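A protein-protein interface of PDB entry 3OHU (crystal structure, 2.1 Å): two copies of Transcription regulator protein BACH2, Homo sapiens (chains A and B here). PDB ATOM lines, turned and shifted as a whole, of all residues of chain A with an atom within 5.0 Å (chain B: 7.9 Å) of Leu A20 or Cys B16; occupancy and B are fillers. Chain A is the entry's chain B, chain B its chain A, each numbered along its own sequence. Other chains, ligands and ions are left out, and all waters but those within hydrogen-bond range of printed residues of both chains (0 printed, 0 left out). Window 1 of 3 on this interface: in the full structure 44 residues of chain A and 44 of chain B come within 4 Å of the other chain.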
ATOM      1  N   CYS A  16      20.019 -17.963 -26.734  1.00  0.00           N
ATOM      2  CA  CYS A  16      19.292 -16.706 -26.534  1.00  0.00           C
ATOM      3  C   CYS A  16      18.983 -16.478 -25.065  1.00  0.00           C
ATOM      4  O   CYS A  16      19.216 -15.396 -24.534  1.00  0.00           O
ATOM      5  CB  CYS A  16      18.029 -16.634 -27.396  1.00  0.00           C
ATOM      6  SG  CYS A  16      18.414 -16.459 -29.164  1.00  0.00           S
ATOM      7  N   THR A  17      18.509 -17.522 -24.405  1.00  0.00           N
ATOM      8  CA  THR A  17      18.207 -17.449 -22.986  1.00  0.00           C
ATOM      9  C   THR A  17      19.457 -17.293 -22.126  1.00  0.00           C
ATOM     10  O   THR A  17      19.440 -16.537 -21.149  1.00  0.00           O
ATOM     11  CB  THR A  17      17.356 -18.651 -22.520  1.00  0.00           C
ATOM     12  OG1 THR A  17      18.162 -19.833 -22.522  1.00  0.00           O
ATOM     13  CG2 THR A  17      16.155 -18.854 -23.459  1.00  0.00           C
ATOM     14  N   ASN A  18      20.540 -17.986 -22.475  1.00  0.00           N
ATOM     15  CA  ASN A  18      21.809 -17.804 -21.735  1.00  0.00           C
ATOM     16  C   ASN A  18      22.437 -16.406 -21.837  1.00  0.00           C
ATOM     17  O   ASN A  18      23.029 -15.930 -20.880  1.00  0.00           O
ATOM     18  CB  ASN A  18      22.846 -18.864 -22.116  1.00  0.00           C
ATOM     19  CG  ASN A  18      22.589 -20.201 -21.443  1.00  0.00           C
ATOM     20  OD1 ASN A  18      21.641 -20.353 -20.658  1.00  0.00           O
ATOM     21  ND2 ASN A  18      23.444 -21.186 -21.745  1.00  0.00           N
ATOM     22  N   ILE A  19      22.343 -15.775 -23.006  1.00  0.00           N
ATOM     23  CA  ILE A  19      22.801 -14.402 -23.176  1.00  0.00           C
ATOM     24  C   ILE A  19      22.041 -13.459 -22.239  1.00  0.00           C
ATOM     25  O   ILE A  19      22.649 -12.710 -21.455  1.00  0.00           O
ATOM     26  CB  ILE A  19      22.603 -13.920 -24.618  1.00  0.00           C
ATOM     27  CG1 ILE A  19      23.558 -14.644 -25.555  1.00  0.00           C
ATOM     28  CG2 ILE A  19      22.798 -12.389 -24.720  1.00  0.00           C
ATOM     29  CD1 ILE A  19      24.998 -14.639 -25.088  1.00  0.00           C
ATOM     30  N   LEU A  20      20.709 -13.504 -22.315  1.00  0.00           N
ATOM     31  CA  LEU A  20      19.884 -12.625 -21.474  1.00  0.00           C
ATOM     32  C   LEU A  20      20.142 -12.845 -20.008  1.00  0.00           C
ATOM     33  O   LEU A  20      20.207 -11.885 -19.236  1.00  0.00           O
ATOM     34  CB  LEU A  20      18.393 -12.724 -21.823  1.00  0.00           C
ATOM     35  CG  LEU A  20      18.238 -11.757 -23.011  1.00  0.00           C
ATOM     36  CD1 LEU A  20      17.398 -12.337 -24.143  1.00  0.00           C
ATOM     37  CD2 LEU A  20      17.744 -10.365 -22.561  1.00  0.00           C
ATOM     38  N   LEU A  21      20.311 -14.104 -19.625  1.00  0.00           N
ATOM     39  CA  LEU A  21      20.746 -14.439 -18.265  1.00  0.00           C
ATOM     40  C   LEU A  21      22.031 -13.691 -17.879  1.00  0.00           C
ATOM     41  O   LEU A  21      22.139 -13.157 -16.774  1.00  0.00           O
ATOM     42  CB  LEU A  21      20.973 -15.947 -18.142  1.00  0.00           C
ATOM     43  CG  LEU A  21      19.850 -16.874 -17.651  1.00  0.00           C
ATOM     44  CD1 LEU A  21      18.456 -16.697 -18.367  1.00  0.00           C
ATOM     45  CD2 LEU A  21      20.335 -18.333 -17.708  1.00  0.00           C
ATOM     46  N   GLY A  22      23.011 -13.696 -18.789  1.00  0.00           N
ATOM     47  CA  GLY A  22      24.257 -12.968 -18.621  1.00  0.00           C
ATOM     48  C   GLY A  22      24.041 -11.471 -18.549  1.00  0.00           C
ATOM     49  O   GLY A  22      24.641 -10.804 -17.720  1.00  0.00           O
ATOM     50  N   LEU A  23      23.173 -10.941 -19.409  1.00  0.00           N
ATOM     51  CA  LEU A  23      22.852  -9.518 -19.387  1.00  0.00           C
ATOM     52  C   LEU A  23      22.217  -9.092 -18.069  1.00  0.00           C
ATOM     53  O   LEU A  23      22.572  -8.044 -17.493  1.00  0.00           O
ATOM     54  CB  LEU A  23      21.990  -9.135 -20.587  1.00  0.00           C
ATOM     55  CG  LEU A  23      22.725  -9.345 -21.923  1.00  0.00           C
ATOM     56  CD1 LEU A  23      21.816  -9.156 -23.147  1.00  0.00           C
ATOM     57  CD2 LEU A  23      23.969  -8.471 -22.022  1.00  0.00           C
ATOM     58  N   ASN A  24      21.300  -9.923 -17.577  1.00  0.00           N
ATOM     59  CA  ASN A  24      20.667  -9.699 -16.280  1.00  0.00           C
ATOM     60  C   ASN A  24      21.632  -9.764 -15.099  1.00  0.00           C
ATOM     61  O   ASN A  24      21.513  -8.972 -14.150  1.00  0.00           O
ATOM     62  CB  ASN A  24      19.532 -10.706 -16.056  1.00  0.00           C
ATOM     63  CG  ASN A  24      18.541 -10.219 -15.031  1.00  0.00           C
ATOM     64  OD1 ASN A  24      18.023  -9.109 -15.140  1.00  0.00           O
ATOM     65  ND2 ASN A  24      18.269 -11.043 -14.038  1.00  0.00           N
ATOM     66  N   ASP A  25      22.572 -10.712 -15.143  1.00  0.00           N
ATOM     67  CA  ASP A  25      23.615 -10.807 -14.117  1.00  0.00           C
ATOM     68  C   ASP A  25      24.428  -9.492 -14.101  1.00  0.00           C
ATOM     69  O   ASP A  25      24.720  -8.956 -13.035  1.00  0.00           O
ATOM     70  CB  ASP A  25      24.515 -12.040 -14.360  1.00  0.00           C
ATOM     71  CG  ASP A  25      25.578 -12.253 -13.257  1.00  0.00           C
ATOM     72  OD1 ASP A  25      25.232 -12.352 -12.058  1.00  0.00           O
ATOM     73  OD2 ASP A  25      26.783 -12.346 -13.590  1.00  0.00           O
ATOM     74  N   VAL A  50      18.836  -3.454 -24.891  1.00  0.00           N
ATOM     75  CA  VAL A  50      17.890  -4.459 -24.448  1.00  0.00           C
ATOM     76  C   VAL A  50      16.484  -3.849 -24.311  1.00  0.00           C
ATOM     77  O   VAL A  50      15.534  -4.346 -24.905  1.00  0.00           O
ATOM     78  CB  VAL A  50      18.338  -5.091 -23.112  1.00  0.00           C
ATOM     79  CG1 VAL A  50      17.236  -5.950 -22.538  1.00  0.00           C
ATOM     80  CG2 VAL A  50      19.606  -5.921 -23.310  1.00  0.00           C
ATOM     81  N   ALA A  90      11.984  -7.859 -19.104  1.00  0.00           N
ATOM     82  CA  ALA A  90      12.691  -7.551 -20.345  1.00  0.00           C
ATOM     83  C   ALA A  90      13.934  -8.427 -20.469  1.00  0.00           C
ATOM     84  O   ALA A  90      14.292  -8.851 -21.561  1.00  0.00           O
ATOM     85  CB  ALA A  90      13.056  -6.076 -20.423  1.00  0.00           C
ATOM     86  N   TYR A  91      14.536  -8.744 -19.327  1.00  0.00           N
ATOM     87  CA  TYR A  91      15.756  -9.537 -19.288  1.00  0.00           C
ATOM     88  C   TYR A  91      15.501 -11.045 -19.191  1.00  0.00           C
ATOM     89  O   TYR A  91      16.216 -11.828 -19.849  1.00  0.00           O
ATOM     90  CB  TYR A  91      16.648  -9.061 -18.125  1.00  0.00           C
ATOM     91  CG  TYR A  91      17.357  -7.752 -18.412  1.00  0.00           C
ATOM     92  CD1 TYR A  91      16.809  -6.532 -18.022  1.00  0.00           C
ATOM     93  CD2 TYR A  91      18.603  -7.741 -19.053  1.00  0.00           C
ATOM     94  CE1 TYR A  91      17.469  -5.333 -18.289  1.00  0.00           C
ATOM     95  CE2 TYR A  91      19.268  -6.555 -19.322  1.00  0.00           C
ATOM     96  CZ  TYR A  91      18.699  -5.357 -18.938  1.00  0.00           C
ATOM     97  OH  TYR A  91      19.366  -4.189 -19.208  1.00  0.00           O
ATOM     98  N   THR A  92      14.497 -11.443 -18.394  1.00  0.00           N
ATOM     99  CA  THR A  92      14.270 -12.855 -18.025  1.00  0.00           C
ATOM    100  C   THR A  92      13.145 -13.570 -18.783  1.00  0.00           C
ATOM    101  O   THR A  92      13.047 -14.803 -18.726  1.00  0.00           O
ATOM    102  CB  THR A  92      13.911 -12.976 -16.548  1.00  0.00           C
ATOM    103  OG1 THR A  92      12.668 -12.288 -16.314  1.00  0.00           O
ATOM    104  CG2 THR A  92      15.021 -12.383 -15.663  1.00  0.00           C
ATOM    105  N   ALA A  93      12.303 -12.795 -19.478  1.00  0.00           N
ATOM    106  CA  ALA A  93      11.078 -13.306 -20.122  1.00  0.00           C
ATOM    107  C   ALA A  93      10.057 -13.829 -19.103  1.00  0.00           C
ATOM    108  O   ALA A  93       9.092 -14.496 -19.479  1.00  0.00           O
ATOM    109  CB  ALA A  93      11.407 -14.402 -21.157  1.00  0.00           C
ATOM    110  N   SER B  12       7.234 -16.071 -21.263  1.00  0.00           N
ATOM    111  CA  SER B  12       7.176 -16.006 -22.708  1.00  0.00           C
ATOM    112  C   SER B  12       8.310 -16.859 -23.261  1.00  0.00           C
ATOM    113  O   SER B  12       9.482 -16.672 -22.920  1.00  0.00           O
ATOM    114  CB  SER B  12       7.269 -14.553 -23.195  1.00  0.00           C
ATOM    115  OG  SER B  12       7.531 -14.490 -24.579  1.00  0.00           O
ATOM    116  N   THR B  13       7.940 -17.799 -24.115  1.00  0.00           N
ATOM    117  CA  THR B  13       8.900 -18.716 -24.706  1.00  0.00           C
ATOM    118  C   THR B  13       9.503 -18.127 -25.991  1.00  0.00           C
ATOM    119  O   THR B  13      10.391 -18.728 -26.601  1.00  0.00           O
ATOM    120  CB  THR B  13       8.256 -20.115 -24.969  1.00  0.00           C
ATOM    121  OG1 THR B  13       7.275 -20.013 -26.010  1.00  0.00           O
ATOM    122  CG2 THR B  13       7.580 -20.652 -23.703  1.00  0.00           C
ATOM    123  N   VAL B  14       9.025 -16.961 -26.415  1.00  0.00           N
ATOM    124  CA  VAL B  14       9.633 -16.311 -27.578  1.00  0.00           C
ATOM    125  C   VAL B  14      10.457 -15.059 -27.195  1.00  0.00           C
ATOM    126  O   VAL B  14      11.303 -14.605 -27.971  1.00  0.00           O
ATOM    127  CB  VAL B  14       8.596 -15.996 -28.694  1.00  0.00           C
ATOM    128  CG1 VAL B  14       7.980 -17.293 -29.250  1.00  0.00           C
ATOM    129  CG2 VAL B  14       7.500 -15.063 -28.175  1.00  0.00           C
ATOM    130  N   HIS B  15      10.209 -14.515 -26.000  1.00  0.00           N
ATOM    131  CA  HIS B  15      10.789 -13.236 -25.611  1.00  0.00           C
ATOM    132  C   HIS B  15      12.294 -13.126 -25.916  1.00  0.00           C
ATOM    133  O   HIS B  15      12.697 -12.262 -26.680  1.00  0.00           O
ATOM    134  CB  HIS B  15      10.541 -12.918 -24.146  1.00  0.00           C
ATOM    135  CG  HIS B  15      11.116 -11.599 -23.726  1.00  0.00           C
ATOM    136  ND1 HIS B  15      10.587 -10.395 -24.145  1.00  0.00           N
ATOM    137  CD2 HIS B  15      12.193 -11.295 -22.964  1.00  0.00           C
ATOM    138  CE1 HIS B  15      11.300  -9.403 -23.637  1.00  0.00           C
ATOM    139  NE2 HIS B  15      12.275  -9.923 -22.911  1.00  0.00           N
ATOM    140  N   CYS B  16      13.095 -14.002 -25.317  1.00  0.00           N
ATOM    141  CA  CYS B  16      14.550 -13.993 -25.472  1.00  0.00           C
ATOM    142  C   CYS B  16      15.040 -14.045 -26.922  1.00  0.00           C
ATOM    143  O   CYS B  16      15.892 -13.267 -27.340  1.00  0.00           O
ATOM    144  CB  CYS B  16      15.155 -15.136 -24.665  1.00  0.00           C
ATOM    145  SG  CYS B  16      14.838 -14.930 -22.916  1.00  0.00           S
ATOM    146  N   THR B  17      14.488 -14.969 -27.674  1.00  0.00           N
ATOM    147  CA  THR B  17      14.739 -15.062 -29.094  1.00  0.00           C
ATOM    148  C   THR B  17      14.437 -13.692 -29.721  1.00  0.00           C
ATOM    149  O   THR B  17      15.214 -13.199 -30.550  1.00  0.00           O
ATOM    150  CB  THR B  17      13.874 -16.186 -29.700  1.00  0.00           C
ATOM    151  OG1 THR B  17      14.225 -17.422 -29.068  1.00  0.00           O
ATOM    152  CG2 THR B  17      14.055 -16.326 -31.233  1.00  0.00           C
ATOM    153  N   ASN B  18      13.321 -13.080 -29.317  1.00  0.00           N
ATOM    154  CA  ASN B  18      12.913 -11.800 -29.910  1.00  0.00           C
ATOM    155  C   ASN B  18      13.878 -10.667 -29.548  1.00  0.00           C
ATOM    156  O   ASN B  18      14.163  -9.805 -30.389  1.00  0.00           O
ATOM    157  CB  ASN B  18      11.452 -11.436 -29.579  1.00  0.00           C
ATOM    158  CG  ASN B  18      10.446 -12.325 -30.298  1.00  0.00           C
ATOM    159  OD1 ASN B  18      10.762 -12.946 -31.316  1.00  0.00           O
ATOM    160  ND2 ASN B  18       9.213 -12.376 -29.778  1.00  0.00           N
ATOM    161  N   ILE B  19      14.406 -10.708 -28.326  1.00  0.00           N
ATOM    162  CA  ILE B  19      15.395  -9.742 -27.892  1.00  0.00           C
ATOM    163  C   ILE B  19      16.694  -9.868 -28.695  1.00  0.00           C
ATOM    164  O   ILE B  19      17.211  -8.871 -29.196  1.00  0.00           O
ATOM    165  CB  ILE B  19      15.718  -9.881 -26.381  1.00  0.00           C
ATOM    166  CG1 ILE B  19      14.566  -9.361 -25.508  1.00  0.00           C
ATOM    167  CG2 ILE B  19      17.053  -9.189 -26.032  1.00  0.00           C
ATOM    168  CD1 ILE B  19      13.808  -8.133 -26.042  1.00  0.00           C
ATOM    169  N   LEU B  20      17.211 -11.090 -28.830  1.00  0.00           N
ATOM    170  CA  LEU B  20      18.400 -11.273 -29.665  1.00  0.00           C
ATOM    171  C   LEU B  20      18.138 -10.871 -31.133  1.00  0.00           C
ATOM    172  O   LEU B  20      18.995 -10.273 -31.782  1.00  0.00           O
ATOM    173  CB  LEU B  20      19.010 -12.683 -29.512  1.00  0.00           C
ATOM    174  CG  LEU B  20      20.534 -12.719 -29.773  1.00  0.00           C
ATOM    175  CD1 LEU B  20      21.314 -11.998 -28.690  1.00  0.00           C
ATOM    176  CD2 LEU B  20      21.048 -14.147 -29.887  1.00  0.00           C
ATOM    177  N   LEU B  21      16.946 -11.147 -31.646  1.00  0.00           N
ATOM    178  CA  LEU B  21      16.604 -10.692 -33.008  1.00  0.00           C
ATOM    179  C   LEU B  21      16.647  -9.138 -33.105  1.00  0.00           C
ATOM    180  O   LEU B  21      17.110  -8.566 -34.104  1.00  0.00           O
ATOM    181  CB  LEU B  21      15.230 -11.230 -33.403  1.00  0.00           C
ATOM    182  CG  LEU B  21      14.731 -11.644 -34.807  1.00  0.00           C
ATOM    183  CD1 LEU B  21      15.640 -12.587 -35.589  1.00  0.00           C
ATOM    184  CD2 LEU B  21      13.341 -12.309 -34.659  1.00  0.00           C
ATOM    185  N   GLY B  22      16.166  -8.468 -32.060  1.00  0.00           N
ATOM    186  CA  GLY B  22      16.190  -7.012 -32.008  1.00  0.00           C
ATOM    187  C   GLY B  22      17.627  -6.489 -31.938  1.00  0.00           C
ATOM    188  O   GLY B  22      17.972  -5.555 -32.651  1.00  0.00           O
ATOM    189  N   LEU B  23      18.445  -7.116 -31.094  1.00  0.00           N
ATOM    190  CA  LEU B  23      19.885  -6.815 -30.963  1.00  0.00           C
ATOM    191  C   LEU B  23      20.675  -6.984 -32.269  1.00  0.00           C
ATOM    192  O   LEU B  23      21.539  -6.159 -32.605  1.00  0.00           O
ATOM    193  CB  LEU B  23      20.497  -7.667 -29.864  1.00  0.00           C
ATOM    194  CG  LEU B  23      20.015  -7.278 -28.463  1.00  0.00           C
ATOM    195  CD1 LEU B  23      20.638  -8.150 -27.435  1.00  0.00           C
ATOM    196  CD2 LEU B  23      20.304  -5.792 -28.155  1.00  0.00           C
ATOM    197  N   ALA B  53      28.878 -11.251 -22.665  1.00  0.00           N
ATOM    198  CA  ALA B  53      27.954 -12.316 -22.282  1.00  0.00           C
ATOM    199  C   ALA B  53      28.160 -13.606 -23.098  1.00  0.00           C
ATOM    200  O   ALA B  53      27.918 -14.702 -22.586  1.00  0.00           O
ATOM    201  CB  ALA B  53      26.500 -11.815 -22.335  1.00  0.00           C
ATOM    202  N   ASN B 116      28.203 -21.551 -25.253  1.00  0.00           N
ATOM    203  CA  ASN B 116      27.010 -22.171 -25.812  1.00  0.00           C
ATOM    204  C   ASN B 116      27.253 -22.983 -27.080  1.00  0.00           C
ATOM    205  O   ASN B 116      26.366 -23.110 -27.930  1.00  0.00           O
ATOM    206  CB  ASN B 116      25.892 -21.131 -25.972  1.00  0.00           C
ATOM    207  CG  ASN B 116      25.717 -20.278 -24.714  1.00  0.00           C
ATOM    208  OD1 ASN B 116      25.851 -20.784 -23.615  1.00  0.00           O
ATOM    209  ND2 ASN B 116      25.487 -18.972 -24.882  1.00  0.00           N
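Cys A16 touches its own counterpart, Cys B16. Cys A16 touches Thr B17, but with the chains exchanged Thr A17 does not touch Cys B16 (4.03 Å). Cys A16 touches Leu B20, and with the chains exchanged Leu A20 touches Cys B16. Leu A20 touches Ile B19, but with the chains exchanged Ile A19 does not touch Leu B20 (4.3 Å). Positions printed for both chains: 16, 17, 18, 19, 20, 21, 22 and 23. Of the 12 pairs that touch across the chains among the printed residues, 3 have their exchanged pair printed and touching as well.
Of the printed residues of chain B, Cys A16 touches Cys B16 (3.98 Å), Thr B17 (3.9 Å) and Leu B20 (3.6 Å). Of chain B, only Cys B16 and Ile B19 come within 4 Å of Leu A20. Printed residues of chain B within 4 Å of Ala A93: Ser B12, His B15 and Cys B16. Of the printed residues of chain A, Ala B53 touches Ile A19 (3.8 Å). The nearest printed residue of chain A that does not touch Ile B19 is Val A50 (4.3 Å).
O of Ala A93 is in hydrogen-bond range of N of Ser B12, 3.0 Å away. O of Ala A90 sits at hydrogen-bond distance from NE2 of His B15, at 2.7 Å. OD1 of Asn B116 lies within hydrogen-bond range of ND2 of Asn A18, at 3.1 Å.
N of Val B14 lies close to OG of Ser B12, 3.4 Å away. The side-chain hydroxyl of Ser B12 is in hydrogen-bond range of the backbone NH of His B15 (3.0 Å).
Cys A16 touches Cys B16. Thr B17 touches Cys A16 (N to CB, 3.9 Å). Leu B20 touches Cys A16. CD1 of Ile A19 touches O of Ala B53 (3.8 Å). CA of Cys B16 touches CD1 of Leu A20 (3.6 Å). Ile B19 touches Leu A20 (CG2 to CD1, 3.7 Å). Ala A90 touches Ile B19 (O to CG1, 3.99 Å). CB of His B15 touches CB of Ala A93, at 3.4 Å. SG of Cys B16 touches CB of Ala A93 (3.9 Å).
Hydrophobic or aromatic side chains of chain B within 4 Å of the printed part of chain A: His B15, Ile B19 and Leu B20. Among the printed residues, 12 pairs touch across the chains. Among the printed residues, no Asp or Glu carboxylate lies within 4 Å of a Lys or Arg side-chain nitrogen of the other chain.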
